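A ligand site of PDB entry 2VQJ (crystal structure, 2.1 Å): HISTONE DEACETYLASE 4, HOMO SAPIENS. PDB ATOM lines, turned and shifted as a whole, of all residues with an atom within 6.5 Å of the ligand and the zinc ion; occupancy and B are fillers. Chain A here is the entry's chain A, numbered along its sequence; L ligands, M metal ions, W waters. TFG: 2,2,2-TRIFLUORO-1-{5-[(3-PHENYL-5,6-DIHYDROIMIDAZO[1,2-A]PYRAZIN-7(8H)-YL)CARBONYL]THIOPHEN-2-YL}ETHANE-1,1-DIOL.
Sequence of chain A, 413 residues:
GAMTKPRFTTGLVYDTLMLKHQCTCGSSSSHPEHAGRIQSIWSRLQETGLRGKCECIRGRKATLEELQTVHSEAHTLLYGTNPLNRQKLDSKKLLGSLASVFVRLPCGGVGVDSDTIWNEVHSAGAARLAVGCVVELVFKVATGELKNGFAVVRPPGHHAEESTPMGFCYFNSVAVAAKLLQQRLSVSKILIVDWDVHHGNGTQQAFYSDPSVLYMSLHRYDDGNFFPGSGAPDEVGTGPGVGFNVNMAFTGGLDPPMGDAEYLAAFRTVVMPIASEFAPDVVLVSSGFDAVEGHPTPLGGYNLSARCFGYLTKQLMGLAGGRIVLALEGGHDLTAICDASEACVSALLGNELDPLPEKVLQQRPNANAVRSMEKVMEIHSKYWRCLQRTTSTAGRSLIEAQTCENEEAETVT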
ATOM      1  N   ARG A  37       1.757  10.801 -11.458  1.00  0.00           N
ATOM      2  CA  ARG A  37       2.545  10.521 -12.648  1.00  0.00           C
ATOM      3  C   ARG A  37       4.026  10.258 -12.355  1.00  0.00           C
ATOM      4  O   ARG A  37       4.545   9.182 -12.672  1.00  0.00           O
ATOM      5  CB  ARG A  37       2.407  11.674 -13.645  1.00  0.00           C
ATOM      6  CG  ARG A  37       0.987  11.851 -14.165  1.00  0.00           C
ATOM      7  CD  ARG A  37       0.738  13.242 -14.682  1.00  0.00           C
ATOM      8  NE  ARG A  37       1.603  13.534 -15.810  1.00  0.00           N
ATOM      9  CZ  ARG A  37       2.550  14.474 -15.845  1.00  0.00           C
ATOM     10  NH1 ARG A  37       2.806  15.263 -14.819  1.00  0.00           N
ATOM     11  NH2 ARG A  37       3.252  14.616 -16.955  1.00  0.00           N
ATOM     12  N   PRO A 156       4.541  20.244 -15.763  1.00  0.00           N
ATOM     13  CA  PRO A 156       5.162  20.602 -17.056  1.00  0.00           C
ATOM     14  C   PRO A 156       5.518  22.067 -17.088  1.00  0.00           C
ATOM     15  O   PRO A 156       5.084  22.807 -16.200  1.00  0.00           O
ATOM     16  CB  PRO A 156       4.059  20.319 -18.088  1.00  0.00           C
ATOM     17  CG  PRO A 156       2.996  19.590 -17.398  1.00  0.00           C
ATOM     18  CD  PRO A 156       3.181  19.693 -15.924  1.00  0.00           C
ATOM     19  N   GLY A 157       6.278  22.506 -18.086  1.00  0.00           N
ATOM     20  CA  GLY A 157       6.642  23.917 -18.199  1.00  0.00           C
ATOM     21  C   GLY A 157       6.469  24.612 -19.549  1.00  0.00           C
ATOM     22  O   GLY A 157       6.509  25.823 -19.612  1.00  0.00           O
ATOM     23  N   HIS A 158       6.262  23.861 -20.624  1.00  0.00           N
ATOM     24  CA  HIS A 158       6.454  24.393 -21.987  1.00  0.00           C
ATOM     25  C   HIS A 158       5.379  25.352 -22.518  1.00  0.00           C
ATOM     26  O   HIS A 158       5.615  26.058 -23.519  1.00  0.00           O
ATOM     27  CB  HIS A 158       6.757  23.256 -22.994  1.00  0.00           C
ATOM     28  CG  HIS A 158       5.592  22.374 -23.313  1.00  0.00           C
ATOM     29  ND1 HIS A 158       5.456  21.763 -24.544  1.00  0.00           N
ATOM     30  CD2 HIS A 158       4.515  21.987 -22.588  1.00  0.00           C
ATOM     31  CE1 HIS A 158       4.358  21.041 -24.553  1.00  0.00           C
ATOM     32  NE2 HIS A 158       3.761  21.162 -23.379  1.00  0.00           N
ATOM     33  N   HIS A 159       4.228  25.417 -21.854  1.00  0.00           N
ATOM     34  CA  HIS A 159       3.180  26.375 -22.189  1.00  0.00           C
ATOM     35  C   HIS A 159       3.337  27.687 -21.420  1.00  0.00           C
ATOM     36  O   HIS A 159       2.705  28.684 -21.795  1.00  0.00           O
ATOM     37  CB  HIS A 159       1.775  25.847 -21.863  1.00  0.00           C
ATOM     38  CG  HIS A 159       1.403  24.568 -22.547  1.00  0.00           C
ATOM     39  ND1 HIS A 159       1.409  24.426 -23.917  1.00  0.00           N
ATOM     40  CD2 HIS A 159       0.945  23.398 -22.048  1.00  0.00           C
ATOM     41  CE1 HIS A 159       1.004  23.208 -24.231  1.00  0.00           C
ATOM     42  NE2 HIS A 159       0.710  22.566 -23.110  1.00  0.00           N
ATOM     43  N   MET A 166      -0.114  28.827 -17.845  1.00  0.00           N
ATOM     44  CA  MET A 166      -1.208  28.205 -18.591  1.00  0.00           C
ATOM     45  C   MET A 166      -0.911  26.746 -18.866  1.00  0.00           C
ATOM     46  O   MET A 166       0.238  26.317 -18.796  1.00  0.00           O
ATOM     47  CB  MET A 166      -1.475  28.914 -19.928  1.00  0.00           C
ATOM     48  CG  MET A 166      -0.230  29.228 -20.719  1.00  0.00           C
ATOM     49  SD  MET A 166      -0.607  30.026 -22.288  1.00  0.00           S
ATOM     50  CE  MET A 166      -1.153  28.588 -23.212  1.00  0.00           C
ATOM     51  N   GLY A 167      -1.959  25.984 -19.161  1.00  0.00           N
ATOM     52  CA  GLY A 167      -1.838  24.556 -19.442  1.00  0.00           C
ATOM     53  C   GLY A 167      -1.093  23.811 -18.347  1.00  0.00           C
ATOM     54  O   GLY A 167      -0.281  22.943 -18.643  1.00  0.00           O
ATOM     55  N   PHE A 168      -1.351  24.163 -17.087  1.00  0.00           N
ATOM     56  CA  PHE A 168      -0.737  23.515 -15.919  1.00  0.00           C
ATOM     57  C   PHE A 168       0.739  23.895 -15.722  1.00  0.00           C
ATOM     58  O   PHE A 168       1.440  23.284 -14.925  1.00  0.00           O
ATOM     59  CB  PHE A 168      -0.899  21.987 -15.965  1.00  0.00           C
ATOM     60  CG  PHE A 168      -2.306  21.526 -16.224  1.00  0.00           C
ATOM     61  CD1 PHE A 168      -2.657  20.952 -17.424  1.00  0.00           C
ATOM     62  CD2 PHE A 168      -3.274  21.670 -15.238  1.00  0.00           C
ATOM     63  CE1 PHE A 168      -3.969  20.530 -17.658  1.00  0.00           C
ATOM     64  CE2 PHE A 168      -4.579  21.263 -15.470  1.00  0.00           C
ATOM     65  CZ  PHE A 168      -4.925  20.689 -16.683  1.00  0.00           C
ATOM     66  N   CYS A 169       1.190  24.916 -16.444  1.00  0.00           N
ATOM     67  CA  CYS A 169       2.578  25.342 -16.416  1.00  0.00           C
ATOM     68  C   CYS A 169       2.706  26.695 -15.744  1.00  0.00           C
ATOM     69  O   CYS A 169       2.031  27.659 -16.136  1.00  0.00           O
ATOM     70  CB  CYS A 169       3.139  25.452 -17.831  1.00  0.00           C
ATOM     71  SG  CYS A 169       3.012  23.913 -18.761  1.00  0.00           S
ATOM     72  N   ASP A 196       6.016  16.533 -26.872  1.00  0.00           N
ATOM     73  CA  ASP A 196       4.702  16.572 -26.254  1.00  0.00           C
ATOM     74  C   ASP A 196       3.700  16.791 -27.388  1.00  0.00           C
ATOM     75  O   ASP A 196       3.999  17.529 -28.340  1.00  0.00           O
ATOM     76  CB  ASP A 196       4.670  17.715 -25.247  1.00  0.00           C
ATOM     77  CG  ASP A 196       3.403  17.742 -24.425  1.00  0.00           C
ATOM     78  OD1 ASP A 196       3.426  17.241 -23.271  1.00  0.00           O
ATOM     79  OD2 ASP A 196       2.390  18.267 -24.923  1.00  0.00           O
ATOM     80  N   VAL A 197       2.516  16.178 -27.327  1.00  0.00           N
ATOM     81  CA  VAL A 197       1.552  16.332 -28.429  1.00  0.00           C
ATOM     82  C   VAL A 197       1.037  17.784 -28.646  1.00  0.00           C
ATOM     83  O   VAL A 197       0.564  18.110 -29.718  1.00  0.00           O
ATOM     84  CB  VAL A 197       0.372  15.303 -28.307  1.00  0.00           C
ATOM     85  CG1 VAL A 197      -0.737  15.768 -27.317  1.00  0.00           C
ATOM     86  CG2 VAL A 197      -0.202  15.010 -29.682  1.00  0.00           C
ATOM     87  N   HIS A 198       1.162  18.637 -27.638  1.00  0.00           N
ATOM     88  CA  HIS A 198       0.705  20.025 -27.713  1.00  0.00           C
ATOM     89  C   HIS A 198       1.867  20.952 -27.972  1.00  0.00           C
ATOM     90  O   HIS A 198       2.984  20.721 -27.496  1.00  0.00           O
ATOM     91  CB  HIS A 198       0.025  20.458 -26.410  1.00  0.00           C
ATOM     92  CG  HIS A 198      -1.080  19.540 -25.981  1.00  0.00           C
ATOM     93  ND1 HIS A 198      -0.876  18.492 -25.119  1.00  0.00           N
ATOM     94  CD2 HIS A 198      -2.389  19.511 -26.313  1.00  0.00           C
ATOM     95  CE1 HIS A 198      -2.012  17.839 -24.954  1.00  0.00           C
ATOM     96  NE2 HIS A 198      -2.951  18.446 -25.652  1.00  0.00           N
ATOM     97  N   HIS A 199       1.634  21.994 -28.762  1.00  0.00           N
ATOM     98  CA  HIS A 199       2.681  22.955 -29.093  1.00  0.00           C
ATOM     99  C   HIS A 199       3.277  23.592 -27.844  1.00  0.00           C
ATOM    100  O   HIS A 199       2.533  23.974 -26.943  1.00  0.00           O
ATOM    101  CB  HIS A 199       2.114  24.042 -30.010  1.00  0.00           C
ATOM    102  CG  HIS A 199       3.112  25.073 -30.401  1.00  0.00           C
ATOM    103  ND1 HIS A 199       2.914  26.418 -30.197  1.00  0.00           N
ATOM    104  CD2 HIS A 199       4.329  24.963 -30.974  1.00  0.00           C
ATOM    105  CE1 HIS A 199       3.960  27.087 -30.647  1.00  0.00           C
ATOM    106  NE2 HIS A 199       4.829  26.228 -31.134  1.00  0.00           N
ATOM    107  N   PHE A 226      -6.546  22.803 -31.931  1.00  0.00           N
ATOM    108  CA  PHE A 226      -6.133  21.924 -30.837  1.00  0.00           C
ATOM    109  C   PHE A 226      -5.285  22.742 -29.852  1.00  0.00           C
ATOM    110  O   PHE A 226      -4.506  23.586 -30.264  1.00  0.00           O
ATOM    111  CB  PHE A 226      -5.354  20.730 -31.426  1.00  0.00           C
ATOM    112  CG  PHE A 226      -5.137  19.590 -30.465  1.00  0.00           C
ATOM    113  CD1 PHE A 226      -6.211  18.800 -30.071  1.00  0.00           C
ATOM    114  CD2 PHE A 226      -3.877  19.288 -29.973  1.00  0.00           C
ATOM    115  CE1 PHE A 226      -6.031  17.758 -29.181  1.00  0.00           C
ATOM    116  CE2 PHE A 226      -3.682  18.248 -29.092  1.00  0.00           C
ATOM    117  CZ  PHE A 226      -4.760  17.479 -28.692  1.00  0.00           C
ATOM    118  N   PHE A 227      -5.466  22.506 -28.551  1.00  0.00           N
ATOM    119  CA  PHE A 227      -4.744  23.277 -27.535  1.00  0.00           C
ATOM    120  C   PHE A 227      -3.222  23.218 -27.734  1.00  0.00           C
ATOM    121  O   PHE A 227      -2.681  22.145 -28.027  1.00  0.00           O
ATOM    122  CB  PHE A 227      -5.083  22.739 -26.134  1.00  0.00           C
ATOM    123  CG  PHE A 227      -4.417  23.503 -25.011  1.00  0.00           C
ATOM    124  CD1 PHE A 227      -5.056  24.597 -24.438  1.00  0.00           C
ATOM    125  CD2 PHE A 227      -3.175  23.114 -24.525  1.00  0.00           C
ATOM    126  CE1 PHE A 227      -4.465  25.306 -23.407  1.00  0.00           C
ATOM    127  CE2 PHE A 227      -2.576  23.817 -23.484  1.00  0.00           C
ATOM    128  CZ  PHE A 227      -3.221  24.924 -22.928  1.00  0.00           C
ATOM    129  N   PRO A 228      -2.518  24.361 -27.537  1.00  0.00           N
ATOM    130  CA  PRO A 228      -2.998  25.706 -27.184  1.00  0.00           C
ATOM    131  C   PRO A 228      -3.485  26.582 -28.333  1.00  0.00           C
ATOM    132  O   PRO A 228      -3.898  27.714 -28.102  1.00  0.00           O
ATOM    133  CB  PRO A 228      -1.770  26.344 -26.528  1.00  0.00           C
ATOM    134  CG  PRO A 228      -0.632  25.734 -27.235  1.00  0.00           C
ATOM    135  CD  PRO A 228      -1.045  24.321 -27.573  1.00  0.00           C
ATOM    136  N   GLY A 288       7.098  15.232 -23.384  1.00  0.00           N
ATOM    137  CA  GLY A 288       5.757  14.820 -23.009  1.00  0.00           C
ATOM    138  C   GLY A 288       5.437  13.511 -23.678  1.00  0.00           C
ATOM    139  O   GLY A 288       5.977  13.192 -24.735  1.00  0.00           O
ATOM    140  N   ASP A 290       2.023  12.403 -24.140  1.00  0.00           N
ATOM    141  CA  ASP A 290       0.606  12.393 -24.456  1.00  0.00           C
ATOM    142  C   ASP A 290       0.271  11.978 -25.897  1.00  0.00           C
ATOM    143  O   ASP A 290      -0.898  11.757 -26.220  1.00  0.00           O
ATOM    144  CB  ASP A 290      -0.107  13.705 -24.032  1.00  0.00           C
ATOM    145  CG  ASP A 290       0.658  14.956 -24.402  1.00  0.00           C
ATOM    146  OD1 ASP A 290       1.695  14.843 -25.091  1.00  0.00           O
ATOM    147  OD2 ASP A 290       0.216  16.074 -23.992  1.00  0.00           O
ATOM    148  N   PRO A 298      -9.602  14.395 -27.104  1.00  0.00           N
ATOM    149  CA  PRO A 298      -9.364  15.762 -26.646  1.00  0.00           C
ATOM    150  C   PRO A 298      -7.969  15.992 -26.059  1.00  0.00           C
ATOM    151  O   PRO A 298      -7.310  16.977 -26.409  1.00  0.00           O
ATOM    152  CB  PRO A 298     -10.457  15.969 -25.592  1.00  0.00           C
ATOM    153  CG  PRO A 298     -10.796  14.624 -25.117  1.00  0.00           C
ATOM    154  CD  PRO A 298     -10.585  13.682 -26.273  1.00  0.00           C
ATOM    155  N   LEU A 299      -7.515  15.084 -25.185  1.00  0.00           N
ATOM    156  CA  LEU A 299      -6.201  15.208 -24.554  1.00  0.00           C
ATOM    157  C   LEU A 299      -5.062  14.924 -25.542  1.00  0.00           C
ATOM    158  O   LEU A 299      -4.063  15.629 -25.552  1.00  0.00           O
ATOM    159  CB  LEU A 299      -6.062  14.251 -23.360  1.00  0.00           C
ATOM    160  CG  LEU A 299      -4.711  14.229 -22.618  1.00  0.00           C
ATOM    161  CD1 LEU A 299      -4.295  15.627 -22.178  1.00  0.00           C
ATOM    162  CD2 LEU A 299      -4.742  13.277 -21.411  1.00  0.00           C
ATOM    163  N   GLU A 329       7.127  16.442 -19.688  1.00  0.00           N
ATOM    164  CA  GLU A 329       6.128  17.493 -19.858  1.00  0.00           C
ATOM    165  C   GLU A 329       4.780  16.825 -19.597  1.00  0.00           C
ATOM    166  O   GLU A 329       4.565  16.354 -18.483  1.00  0.00           O
ATOM    167  CB  GLU A 329       6.218  18.091 -21.257  1.00  0.00           C
ATOM    168  CG  GLU A 329       7.543  18.740 -21.558  1.00  0.00           C
ATOM    169  CD  GLU A 329       7.729  20.106 -20.900  1.00  0.00           C
ATOM    170  OE1 GLU A 329       6.825  20.563 -20.160  1.00  0.00           O
ATOM    171  OE2 GLU A 329       8.784  20.725 -21.123  1.00  0.00           O
ATOM    172  N   GLY A 330       3.907  16.736 -20.610  1.00  0.00           N
ATOM    173  CA  GLY A 330       2.614  16.079 -20.511  1.00  0.00           C
ATOM    174  C   GLY A 330       2.621  14.577 -20.655  1.00  0.00           C
ATOM    175  O   GLY A 330       3.670  13.915 -20.616  1.00  0.00           O
ATOM    176  N   GLY A 331       1.432  14.015 -20.804  1.00  0.00           N
ATOM    177  CA  GLY A 331       1.225  12.584 -20.695  1.00  0.00           C
ATOM    178  C   GLY A 331       0.488  12.329 -19.390  1.00  0.00           C
ATOM    179  O   GLY A 331       0.819  12.932 -18.383  1.00  0.00           O
HETATM  180  C14 TFG L   1     -12.046  20.781 -19.923  1.00  0.00           C
HETATM  181  C15 TFG L   1     -13.235  20.258 -20.396  1.00  0.00           C
HETATM  182  C16 TFG L   1     -13.226  19.284 -21.399  1.00  0.00           C
HETATM  183  C17 TFG L   1     -12.027  18.839 -21.937  1.00  0.00           C
HETATM  184  C18 TFG L   1     -10.832  19.371 -21.454  1.00  0.00           C
HETATM  185  C13 TFG L   1     -10.831  20.332 -20.446  1.00  0.00           C
HETATM  186  C19 TFG L   1      -9.641  20.897 -19.989  1.00  0.00           C
HETATM  187  C12 TFG L   1      -9.286  21.399 -18.802  1.00  0.00           C
HETATM  188  N3  TFG L   1      -8.034  21.862 -18.877  1.00  0.00           N
HETATM  189  C11 TFG L   1      -7.569  21.703 -20.114  1.00  0.00           C
HETATM  190  C10 TFG L   1      -6.200  22.084 -20.700  1.00  0.00           C
HETATM  191  N2  TFG L   1      -8.588  21.088 -20.859  1.00  0.00           N
HETATM  192  C9  TFG L   1      -8.459  20.721 -22.274  1.00  0.00           C
HETATM  193  C8  TFG L   1      -7.327  21.498 -22.881  1.00  0.00           C
HETATM  194  N1  TFG L   1      -6.133  21.453 -22.021  1.00  0.00           N
HETATM  195  C7  TFG L   1      -5.092  20.789 -22.507  1.00  0.00           C
HETATM  196  O1  TFG L   1      -5.258  20.344 -23.639  1.00  0.00           O
HETATM  197  C4  TFG L   1      -3.691  20.649 -21.928  1.00  0.00           C
HETATM  198  S1  TFG L   1      -2.652  19.436 -22.430  1.00  0.00           S
HETATM  199  C3  TFG L   1      -3.017  21.488 -21.132  1.00  0.00           C
HETATM  200  C2  TFG L   1      -1.724  21.118 -20.902  1.00  0.00           C
HETATM  201  C1  TFG L   1      -1.329  19.982 -21.532  1.00  0.00           C
HETATM  202  C5  TFG L   1       0.053  19.273 -21.543  1.00  0.00           C
HETATM  203  C6  TFG L   1       0.949  19.609 -20.347  1.00  0.00           C
HETATM  204  F1  TFG L   1       1.061  20.924 -20.196  1.00  0.00           F
HETATM  205  F2  TFG L   1       0.479  19.032 -19.270  1.00  0.00           F
HETATM  206  F3  TFG L   1       2.146  19.110 -20.577  1.00  0.00           F
HETATM  207  O3  TFG L   1      -0.100  17.850 -21.641  1.00  0.00           O
HETATM  208  O2  TFG L   1       0.783  19.676 -22.745  1.00  0.00           O
HETATM  209 ZN    ZN M   1       0.661  17.961 -23.893  1.00  0.00          ZN
HETATM  210  O   HOH W   1      -7.043  24.073 -17.914  1.00  0.00           O
HETATM  211  O   HOH W   2      -0.732  15.698 -20.701  1.00  0.00           O
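Of the 23 residues printed, 3 come within 4 Å of the zinc ion.
The nearest printed residue that does not touch the zinc ion is Val 197 (4.3 Å).
The side-chain sulfur (SG) of Cys 169 is in hydrogen-bond range of the backbone carbonyl oxygen (O) of Pro 156, at 3.5 Å.
The side-chain sulfur of Cys 169 lies close to the backbone NH of Gly 157, 3.6 Å away.
The side-chain sulfur (SG) of Cys 169 is in hydrogen-bond range of the backbone NH (N) of His 159, at 3.6 Å.
O of Leu 299 is in hydrogen-bond range of NE2 of His 198, at 3.0 Å.
The backbone carbonyl oxygen (O) of Glu 329 sits at hydrogen-bond distance from the guanidinium group (NH2) of Arg 37, 2.7 Å away.
NE2 of His 159 lies within hydrogen-bond range of NE2 of His 158.
The backbone carbonyl oxygen (O) of His 199 sits close to a ring nitrogen (ND1) of His 159, at 3.3 Å.
N of His 158 sits at hydrogen-bond distance from OE1 of Glu 329 (3.4 Å).
The zinc ion is bound by the side-chain carboxylate of Asp 290, the side-chain carboxylate of Asp 196, a ring nitrogen (ND1) of His 198, an oxygen (O2) of the ligand and an oxygen (O3) of the ligand.
The zinc ion has five donor atoms within binding distance.
NE2 of His 159 lies close to O2 of the ligand.
NE2 of His 158 lies close to O2 of the ligand (3.4 Å).
A fluorine (F1) of the ligand lies close to the backbone carbonyl oxygen of Gly 167.
F3 of the ligand sits close to N of Gly 330, 3.0 Å away.
Pro 156 touches the ligand (CG to F2, 3.2 Å).
Phe 168 touches the ligand (CD1 to C2, 3.6 Å).
Cys 169 touches the ligand.
Phe 227 touches the ligand (CE2 to C3, 3.3 Å).
C of Glu 329 touches F3 of the ligand, 3.6 Å away.
Hydrophobic or aromatic side chains within 4 Å of the ligand: Pro 156, His 159, Phe 168, His 198 and Phe 227.
12 residues have an atom within 4 Å of the ligand: Pro 156, His 158, His 159, Gly 167, Phe 168, Cys 169, Asp 196, His 198, Phe 227, Asp 290, Glu 329 and Gly 330.
Along chain A the residues within 4 Å of the ligand span positions 156 to 330.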
